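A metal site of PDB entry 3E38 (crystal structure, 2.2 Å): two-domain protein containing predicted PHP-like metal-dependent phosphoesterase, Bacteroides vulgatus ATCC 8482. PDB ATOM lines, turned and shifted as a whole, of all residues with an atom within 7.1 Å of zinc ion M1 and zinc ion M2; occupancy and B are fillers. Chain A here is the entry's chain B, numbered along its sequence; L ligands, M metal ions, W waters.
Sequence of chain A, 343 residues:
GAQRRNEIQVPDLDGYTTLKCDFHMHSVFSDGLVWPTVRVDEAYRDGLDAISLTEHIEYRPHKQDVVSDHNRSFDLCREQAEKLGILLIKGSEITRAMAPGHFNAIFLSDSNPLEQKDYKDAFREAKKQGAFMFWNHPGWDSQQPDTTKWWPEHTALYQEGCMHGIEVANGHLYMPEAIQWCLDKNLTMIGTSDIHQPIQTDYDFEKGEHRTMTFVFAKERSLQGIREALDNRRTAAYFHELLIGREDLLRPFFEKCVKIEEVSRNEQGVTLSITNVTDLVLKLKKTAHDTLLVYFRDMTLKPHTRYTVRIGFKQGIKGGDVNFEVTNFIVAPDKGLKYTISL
The side-chain carboxylate of Glu 167 sits at hydrogen-bond distance from the backbone NH of His 137.
The backbone NH (N) of Glu 93 sits at hydrogen-bond distance from the backbone carbonyl oxygen (O) of Glu 55, at 2.8 Å.
N of His 26 lies within hydrogen-bond range of O of Ile 195 (2.9 Å).
O of Glu 93 is in hydrogen-bond range of OG1 of Thr 95 (2.9 Å).
ND1 of His 26 sits close to OD1 of Asp 31 (3.4 Å).
ND1 of His 56 lies close to OE1 of Glu 93 (3.2 Å).
OD2 of Asp 194 is in hydrogen-bond range of ND2 of Asn 170 (3.0 Å).
A ring nitrogen (ND1) of His 24 sits at hydrogen-bond distance from the side-chain carboxylate (OE2) of Glu 167, at 2.8 Å.
Residues that only touch zinc ion M1: His 56 (3.97 Å).
Within 4 Å of zinc ion M1: His 24, His 26, His 56, Glu 93 and Asp 194.
The nearest printed residue that does not touch zinc ion M1 is His 196 (4.2 Å).
Within 4 Å of zinc ion M2: Glu 93, His 102 and His 137.
Along chain A the residues within 4 Å of zinc ion M2 span positions 93 to 137.
Zinc ion M1 is bound by O1 of the ligand (1.9 Å).
Zinc ion M1 is bound by water W1 (2.1 Å).
Zinc ion M1 is bound by NE2 of His 24 (2.2 Å).
Zinc ion M1 is bound by a ring nitrogen (NE2) of His 26 (2.2 Å).
The side-chain carboxylate (OE1) of Glu 93 is bound to zinc ion M1 (2.2 Å).
Zinc ion M1 is bound by OD1 of Asp 194 (2.5 Å).
Zinc ion M1 has six donor atoms within binding distance.
Zinc ion M2 is bound by water W1 (1.8 Å), O2 of the ligand (1.9 Å), NE2 of His 137 (2.2 Å), OE2 of Glu 93 (2.2 Å) and ND1 of His 102 (2.3 Å).
Zinc ion M2 has five donor atoms within binding distance.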
ATOM      1  N   HIS A  24       8.818  -2.170  -0.665  1.00  0.00           N
ATOM      2  CA  HIS A  24       8.580  -0.907   0.048  1.00  0.00           C
ATOM      3  C   HIS A  24       7.246  -0.297  -0.307  1.00  0.00           C
ATOM      4  O   HIS A  24       7.000   0.177  -1.404  1.00  0.00           O
ATOM      5  CB  HIS A  24       9.701   0.074  -0.324  1.00  0.00           C
ATOM      6  CG  HIS A  24       9.750   1.313   0.490  1.00  0.00           C
ATOM      7  ND1 HIS A  24      10.891   2.092   0.551  1.00  0.00           N
ATOM      8  CD2 HIS A  24       8.861   1.878   1.339  1.00  0.00           C
ATOM      9  CE1 HIS A  24      10.685   3.114   1.367  1.00  0.00           C
ATOM     10  NE2 HIS A  24       9.460   3.018   1.850  1.00  0.00           N
ATOM     11  N   MET A  25       6.370  -0.332   0.669  1.00  0.00           N
ATOM     12  CA  MET A  25       5.046   0.215   0.494  1.00  0.00           C
ATOM     13  C   MET A  25       4.373   0.419   1.832  1.00  0.00           C
ATOM     14  O   MET A  25       4.840  -0.101   2.854  1.00  0.00           O
ATOM     15  CB  MET A  25       4.231  -0.711  -0.387  1.00  0.00           C
ATOM     16  CG  MET A  25       3.913  -2.029   0.244  1.00  0.00           C
ATOM     17  SD  MET A  25       3.115  -3.278  -1.033  1.00  0.00           S
ATOM     18  CE  MET A  25       4.583  -3.321  -2.255  1.00  0.00           C
ATOM     19  N   HIS A  26       3.232   1.093   1.763  1.00  0.00           N
ATOM     20  CA  HIS A  26       2.468   1.535   2.940  1.00  0.00           C
ATOM     21  C   HIS A  26       0.978   1.385   2.899  1.00  0.00           C
ATOM     22  O   HIS A  26       0.386   1.367   1.850  1.00  0.00           O
ATOM     23  CB  HIS A  26       2.777   2.990   3.195  1.00  0.00           C
ATOM     24  CG  HIS A  26       4.228   3.258   3.385  1.00  0.00           C
ATOM     25  ND1 HIS A  26       4.843   3.233   4.619  1.00  0.00           N
ATOM     26  CD2 HIS A  26       5.208   3.505   2.477  1.00  0.00           C
ATOM     27  CE1 HIS A  26       6.135   3.508   4.463  1.00  0.00           C
ATOM     28  NE2 HIS A  26       6.367   3.696   3.172  1.00  0.00           N
ATOM     29  N   ASP A  31       1.316   5.679   7.068  1.00  0.00           N
ATOM     30  CA  ASP A  31       0.886   6.889   6.307  1.00  0.00           C
ATOM     31  C   ASP A  31       0.326   6.555   4.931  1.00  0.00           C
ATOM     32  O   ASP A  31       0.028   7.408   4.137  1.00  0.00           O
ATOM     33  CB  ASP A  31       2.025   7.950   6.218  1.00  0.00           C
ATOM     34  CG  ASP A  31       3.240   7.473   5.435  1.00  0.00           C
ATOM     35  OD1 ASP A  31       3.342   6.261   5.246  1.00  0.00           O
ATOM     36  OD2 ASP A  31       4.141   8.299   5.031  1.00  0.00           O
ATOM     37  N   THR A  54       5.952  -2.369   4.302  1.00  0.00           N
ATOM     38  CA  THR A  54       6.958  -1.822   5.186  1.00  0.00           C
ATOM     39  C   THR A  54       6.511  -0.518   5.808  1.00  0.00           C
ATOM     40  O   THR A  54       6.941   0.543   5.421  1.00  0.00           O
ATOM     41  CB  THR A  54       8.266  -1.574   4.421  1.00  0.00           C
ATOM     42  OG1 THR A  54       8.081  -0.524   3.476  1.00  0.00           O
ATOM     43  CG2 THR A  54       8.729  -2.851   3.732  1.00  0.00           C
ATOM     44  N   GLU A  55       5.685  -0.648   6.843  1.00  0.00           N
ATOM     45  CA  GLU A  55       5.145   0.505   7.563  1.00  0.00           C
ATOM     46  C   GLU A  55       6.273   1.253   8.296  1.00  0.00           C
ATOM     47  O   GLU A  55       7.300   0.698   8.702  1.00  0.00           O
ATOM     48  CB  GLU A  55       4.065   0.125   8.582  1.00  0.00           C
ATOM     49  CG  GLU A  55       2.914  -0.834   8.163  1.00  0.00           C
ATOM     50  CD  GLU A  55       1.972  -0.366   7.069  1.00  0.00           C
ATOM     51  OE1 GLU A  55       2.129   0.749   6.523  1.00  0.00           O
ATOM     52  OE2 GLU A  55       1.039  -1.149   6.761  1.00  0.00           O
ATOM     53  N   HIS A  56       6.051   2.551   8.427  1.00  0.00           N
ATOM     54  CA  HIS A  56       6.948   3.379   9.216  1.00  0.00           C
ATOM     55  C   HIS A  56       6.798   2.888  10.640  1.00  0.00           C
ATOM     56  O   HIS A  56       5.686   2.645  11.118  1.00  0.00           O
ATOM     57  CB  HIS A  56       6.565   4.869   9.205  1.00  0.00           C
ATOM     58  CG  HIS A  56       6.713   5.533   7.878  1.00  0.00           C
ATOM     59  ND1 HIS A  56       7.949   5.916   7.371  1.00  0.00           N
ATOM     60  CD2 HIS A  56       5.797   5.921   6.965  1.00  0.00           C
ATOM     61  CE1 HIS A  56       7.771   6.485   6.198  1.00  0.00           C
ATOM     62  NE2 HIS A  56       6.477   6.488   5.922  1.00  0.00           N
ATOM     63  N   GLU A  93       9.896   0.164   7.946  1.00  0.00           N
ATOM     64  CA  GLU A  93      10.644   1.366   7.619  1.00  0.00           C
ATOM     65  C   GLU A  93      11.061   2.188   8.823  1.00  0.00           C
ATOM     66  O   GLU A  93      10.251   2.835   9.503  1.00  0.00           O
ATOM     67  CB  GLU A  93       9.858   2.261   6.635  1.00  0.00           C
ATOM     68  CG  GLU A  93      10.789   3.342   6.079  1.00  0.00           C
ATOM     69  CD  GLU A  93      10.148   4.244   5.091  1.00  0.00           C
ATOM     70  OE1 GLU A  93       8.898   4.276   4.822  1.00  0.00           O
ATOM     71  OE2 GLU A  93      10.935   4.937   4.533  1.00  0.00           O
ATOM     72  N   ILE A  94      12.377   2.162   9.047  1.00  0.00           N
ATOM     73  CA  ILE A  94      13.040   2.903  10.144  1.00  0.00           C
ATOM     74  C   ILE A  94      13.214   4.268   9.525  1.00  0.00           C
ATOM     75  O   ILE A  94      13.968   4.467   8.589  1.00  0.00           O
ATOM     76  CB  ILE A  94      14.393   2.283  10.577  1.00  0.00           C
ATOM     77  CG1 ILE A  94      14.222   0.803  10.923  1.00  0.00           C
ATOM     78  CG2 ILE A  94      15.011   3.054  11.728  1.00  0.00           C
ATOM     79  CD1 ILE A  94      15.562  -0.009  10.935  1.00  0.00           C
ATOM     80  N   THR A  95      12.409   5.176  10.055  1.00  0.00           N
ATOM     81  CA  THR A  95      12.206   6.503   9.573  1.00  0.00           C
ATOM     82  C   THR A  95      12.847   7.464  10.523  1.00  0.00           C
ATOM     83  O   THR A  95      12.359   7.698  11.626  1.00  0.00           O
ATOM     84  CB  THR A  95      10.661   6.806   9.502  1.00  0.00           C
ATOM     85  OG1 THR A  95       9.928   5.700   8.932  1.00  0.00           O
ATOM     86  CG2 THR A  95      10.397   8.062   8.711  1.00  0.00           C
ATOM     87  N   GLY A 101      18.868   8.916   7.780  1.00  0.00           N
ATOM     88  CA  GLY A 101      17.693   9.022   6.947  1.00  0.00           C
ATOM     89  C   GLY A 101      16.751   7.880   7.166  1.00  0.00           C
ATOM     90  O   GLY A 101      16.492   7.493   8.286  1.00  0.00           O
ATOM     91  N   HIS A 102      16.216   7.356   6.072  1.00  0.00           N
ATOM     92  CA  HIS A 102      15.247   6.232   6.128  1.00  0.00           C
ATOM     93  C   HIS A 102      15.815   4.970   5.536  1.00  0.00           C
ATOM     94  O   HIS A 102      16.366   4.992   4.434  1.00  0.00           O
ATOM     95  CB  HIS A 102      14.004   6.541   5.292  1.00  0.00           C
ATOM     96  CG  HIS A 102      13.259   7.768   5.702  1.00  0.00           C
ATOM     97  ND1 HIS A 102      11.953   7.981   5.343  1.00  0.00           N
ATOM     98  CD2 HIS A 102      13.632   8.844   6.431  1.00  0.00           C
ATOM     99  CE1 HIS A 102      11.551   9.150   5.826  1.00  0.00           C
ATOM    100  NE2 HIS A 102      12.542   9.685   6.507  1.00  0.00           N
ATOM    101  N   PHE A 103      15.660   3.875   6.265  1.00  0.00           N
ATOM    102  CA  PHE A 103      16.049   2.519   5.814  1.00  0.00           C
ATOM    103  C   PHE A 103      14.899   1.537   5.987  1.00  0.00           C
ATOM    104  O   PHE A 103      14.127   1.647   6.893  1.00  0.00           O
ATOM    105  CB  PHE A 103      17.186   1.933   6.636  1.00  0.00           C
ATOM    106  CG  PHE A 103      18.575   2.510   6.353  1.00  0.00           C
ATOM    107  CD1 PHE A 103      18.835   3.843   6.521  1.00  0.00           C
ATOM    108  CD2 PHE A 103      19.620   1.677   5.956  1.00  0.00           C
ATOM    109  CE1 PHE A 103      20.094   4.363   6.248  1.00  0.00           C
ATOM    110  CE2 PHE A 103      20.867   2.174   5.668  1.00  0.00           C
ATOM    111  CZ  PHE A 103      21.110   3.529   5.821  1.00  0.00           C
ATOM    112  N   ASN A 104      14.864   0.550   5.110  1.00  0.00           N
ATOM    113  CA  ASN A 104      13.965  -0.580   5.264  1.00  0.00           C
ATOM    114  C   ASN A 104      14.727  -1.806   5.734  1.00  0.00           C
ATOM    115  O   ASN A 104      15.821  -2.083   5.291  1.00  0.00           O
ATOM    116  CB  ASN A 104      13.218  -0.911   3.993  1.00  0.00           C
ATOM    117  CG  ASN A 104      11.959  -0.091   3.847  1.00  0.00           C
ATOM    118  OD1 ASN A 104      11.787   0.928   4.490  1.00  0.00           O
ATOM    119  ND2 ASN A 104      11.060  -0.554   2.992  1.00  0.00           N
ATOM    120  N   ASN A 136      16.773   3.733   1.904  1.00  0.00           N
ATOM    121  CA  ASN A 136      15.674   4.266   1.095  1.00  0.00           C
ATOM    122  C   ASN A 136      15.915   5.694   0.574  1.00  0.00           C
ATOM    123  O   ASN A 136      16.440   6.550   1.253  1.00  0.00           O
ATOM    124  CB  ASN A 136      14.333   4.272   1.864  1.00  0.00           C
ATOM    125  CG  ASN A 136      13.955   2.931   2.401  1.00  0.00           C
ATOM    126  OD1 ASN A 136      14.328   1.893   1.870  1.00  0.00           O
ATOM    127  ND2 ASN A 136      13.206   2.937   3.489  1.00  0.00           N
ATOM    128  N   HIS A 137      15.463   5.896  -0.664  1.00  0.00           N
ATOM    129  CA  HIS A 137      15.499   7.204  -1.309  1.00  0.00           C
ATOM    130  C   HIS A 137      16.624   8.104  -0.832  1.00  0.00           C
ATOM    131  O   HIS A 137      16.389   9.133  -0.243  1.00  0.00           O
ATOM    132  CB  HIS A 137      14.147   7.927  -1.155  1.00  0.00           C
ATOM    133  CG  HIS A 137      13.529   7.838   0.202  1.00  0.00           C
ATOM    134  ND1 HIS A 137      14.003   8.545   1.295  1.00  0.00           N
ATOM    135  CD2 HIS A 137      12.422   7.180   0.635  1.00  0.00           C
ATOM    136  CE1 HIS A 137      13.228   8.290   2.334  1.00  0.00           C
ATOM    137  NE2 HIS A 137      12.286   7.450   1.973  1.00  0.00           N
ATOM    138  N   TRP A 140      15.983  11.639  -2.066  1.00  0.00           N
ATOM    139  CA  TRP A 140      14.746  12.396  -1.744  1.00  0.00           C
ATOM    140  C   TRP A 140      15.171  13.787  -1.328  1.00  0.00           C
ATOM    141  O   TRP A 140      15.918  13.957  -0.364  1.00  0.00           O
ATOM    142  CB  TRP A 140      14.016  11.711  -0.631  1.00  0.00           C
ATOM    143  CG  TRP A 140      12.692  12.272  -0.232  1.00  0.00           C
ATOM    144  CD1 TRP A 140      11.711  12.773  -1.056  1.00  0.00           C
ATOM    145  CD2 TRP A 140      12.119  12.215   1.074  1.00  0.00           C
ATOM    146  NE1 TRP A 140      10.593  13.097  -0.323  1.00  0.00           N
ATOM    147  CE2 TRP A 140      10.814  12.749   0.990  1.00  0.00           C
ATOM    148  CE3 TRP A 140      12.595  11.781   2.329  1.00  0.00           C
ATOM    149  CZ2 TRP A 140       9.975  12.862   2.107  1.00  0.00           C
ATOM    150  CZ3 TRP A 140      11.774  11.905   3.434  1.00  0.00           C
ATOM    151  CH2 TRP A 140      10.475  12.429   3.310  1.00  0.00           C
ATOM    152  N   GLN A 143      15.176  15.626   2.274  1.00  0.00           N
ATOM    153  CA  GLN A 143      16.237  15.397   3.245  1.00  0.00           C
ATOM    154  C   GLN A 143      17.621  15.757   2.681  1.00  0.00           C
ATOM    155  O   GLN A 143      18.559  15.999   3.437  1.00  0.00           O
ATOM    156  CB  GLN A 143      16.170  13.952   3.768  1.00  0.00           C
ATOM    157  CG  GLN A 143      15.020  13.726   4.741  1.00  0.00           C
ATOM    158  CD  GLN A 143      15.174  12.449   5.551  1.00  0.00           C
ATOM    159  OE1 GLN A 143      15.726  11.463   5.081  1.00  0.00           O
ATOM    160  NE2 GLN A 143      14.688  12.466   6.773  1.00  0.00           N
ATOM    161  N   GLU A 167      18.217   1.792  -2.487  1.00  0.00           N
ATOM    162  CA  GLU A 167      17.220   2.093  -3.512  1.00  0.00           C
ATOM    163  C   GLU A 167      17.861   2.996  -4.547  1.00  0.00           C
ATOM    164  O   GLU A 167      18.408   4.075  -4.223  1.00  0.00           O
ATOM    165  CB  GLU A 167      15.998   2.755  -2.923  1.00  0.00           C
ATOM    166  CG  GLU A 167      15.110   1.793  -2.177  1.00  0.00           C
ATOM    167  CD  GLU A 167      13.801   2.451  -1.698  1.00  0.00           C
ATOM    168  OE1 GLU A 167      13.796   3.703  -1.574  1.00  0.00           O
ATOM    169  OE2 GLU A 167      12.814   1.712  -1.391  1.00  0.00           O
ATOM    170  N   ASN A 170      13.001   4.925  -6.564  1.00  0.00           N
ATOM    171  CA  ASN A 170      11.828   4.971  -5.662  1.00  0.00           C
ATOM    172  C   ASN A 170      10.665   5.728  -6.312  1.00  0.00           C
ATOM    173  O   ASN A 170      10.729   6.932  -6.524  1.00  0.00           O
ATOM    174  CB  ASN A 170      12.210   5.621  -4.324  1.00  0.00           C
ATOM    175  CG  ASN A 170      11.128   5.520  -3.249  1.00  0.00           C
ATOM    176  OD1 ASN A 170      10.043   6.020  -3.448  1.00  0.00           O
ATOM    177  ND2 ASN A 170      11.452   4.928  -2.088  1.00  0.00           N
ATOM    178  N   ASP A 194       7.219   2.474  -2.982  1.00  0.00           N
ATOM    179  CA  ASP A 194       7.055   3.370  -1.844  1.00  0.00           C
ATOM    180  C   ASP A 194       5.627   3.920  -1.896  1.00  0.00           C
ATOM    181  O   ASP A 194       5.323   5.033  -1.500  1.00  0.00           O
ATOM    182  CB  ASP A 194       8.118   4.488  -1.853  1.00  0.00           C
ATOM    183  CG  ASP A 194       8.303   5.121  -0.483  1.00  0.00           C
ATOM    184  OD1 ASP A 194       7.470   4.785   0.400  1.00  0.00           O
ATOM    185  OD2 ASP A 194       9.284   5.899  -0.253  1.00  0.00           O
ATOM    186  N   ILE A 195       4.741   3.071  -2.410  1.00  0.00           N
ATOM    187  CA  ILE A 195       3.326   3.451  -2.603  1.00  0.00           C
ATOM    188  C   ILE A 195       2.576   3.769  -1.317  1.00  0.00           C
ATOM    189  O   ILE A 195       2.648   3.025  -0.378  1.00  0.00           O
ATOM    190  CB  ILE A 195       2.549   2.373  -3.458  1.00  0.00           C
ATOM    191  CG1 ILE A 195       1.205   2.934  -3.895  1.00  0.00           C
ATOM    192  CG2 ILE A 195       2.498   1.005  -2.764  1.00  0.00           C
ATOM    193  CD1 ILE A 195       1.345   3.997  -5.033  1.00  0.00           C
ATOM    194  N   HIS A 196       1.890   4.931  -1.328  1.00  0.00           N
ATOM    195  CA  HIS A 196       0.982   5.379  -0.232  1.00  0.00           C
ATOM    196  C   HIS A 196      -0.450   5.428  -0.733  1.00  0.00           C
ATOM    197  O   HIS A 196      -1.383   4.995  -0.075  1.00  0.00           O
ATOM    198  CB  HIS A 196       1.362   6.749   0.342  1.00  0.00           C
ATOM    199  CG  HIS A 196       2.690   6.781   1.042  1.00  0.00           C
ATOM    200  ND1 HIS A 196       3.884   6.531   0.381  1.00  0.00           N
ATOM    201  CD2 HIS A 196       3.022   7.054   2.326  1.00  0.00           C
ATOM    202  CE1 HIS A 196       4.891   6.639   1.241  1.00  0.00           C
ATOM    203  NE2 HIS A 196       4.406   6.976   2.420  1.00  0.00           N
HETATM  204 AS1  LIG L   1       7.903   8.021   3.052  1.00  0.00          AS
HETATM  205  O1  LIG L   1       7.447   6.319   3.259  1.00  0.00           O
HETATM  206  O2  LIG L   1       9.518   8.250   3.697  1.00  0.00           O
HETATM  207  C1  LIG L   1       8.092   8.401   1.111  1.00  0.00           C
HETATM  208  C2  LIG L   1       6.751   9.288   3.985  1.00  0.00           C
HETATM  209 ZN    ZN M   1       8.313   4.662   2.713  1.00  0.00          ZN
HETATM  210 ZN    ZN M   2      10.895   6.937   3.599  1.00  0.00          ZN
HETATM  211 ZN    ZN M   3       5.402   7.275   4.242  1.00  0.00          ZN
HETATM  212  O   HOH W   1      10.088   5.784   2.456  1.00  0.00           O
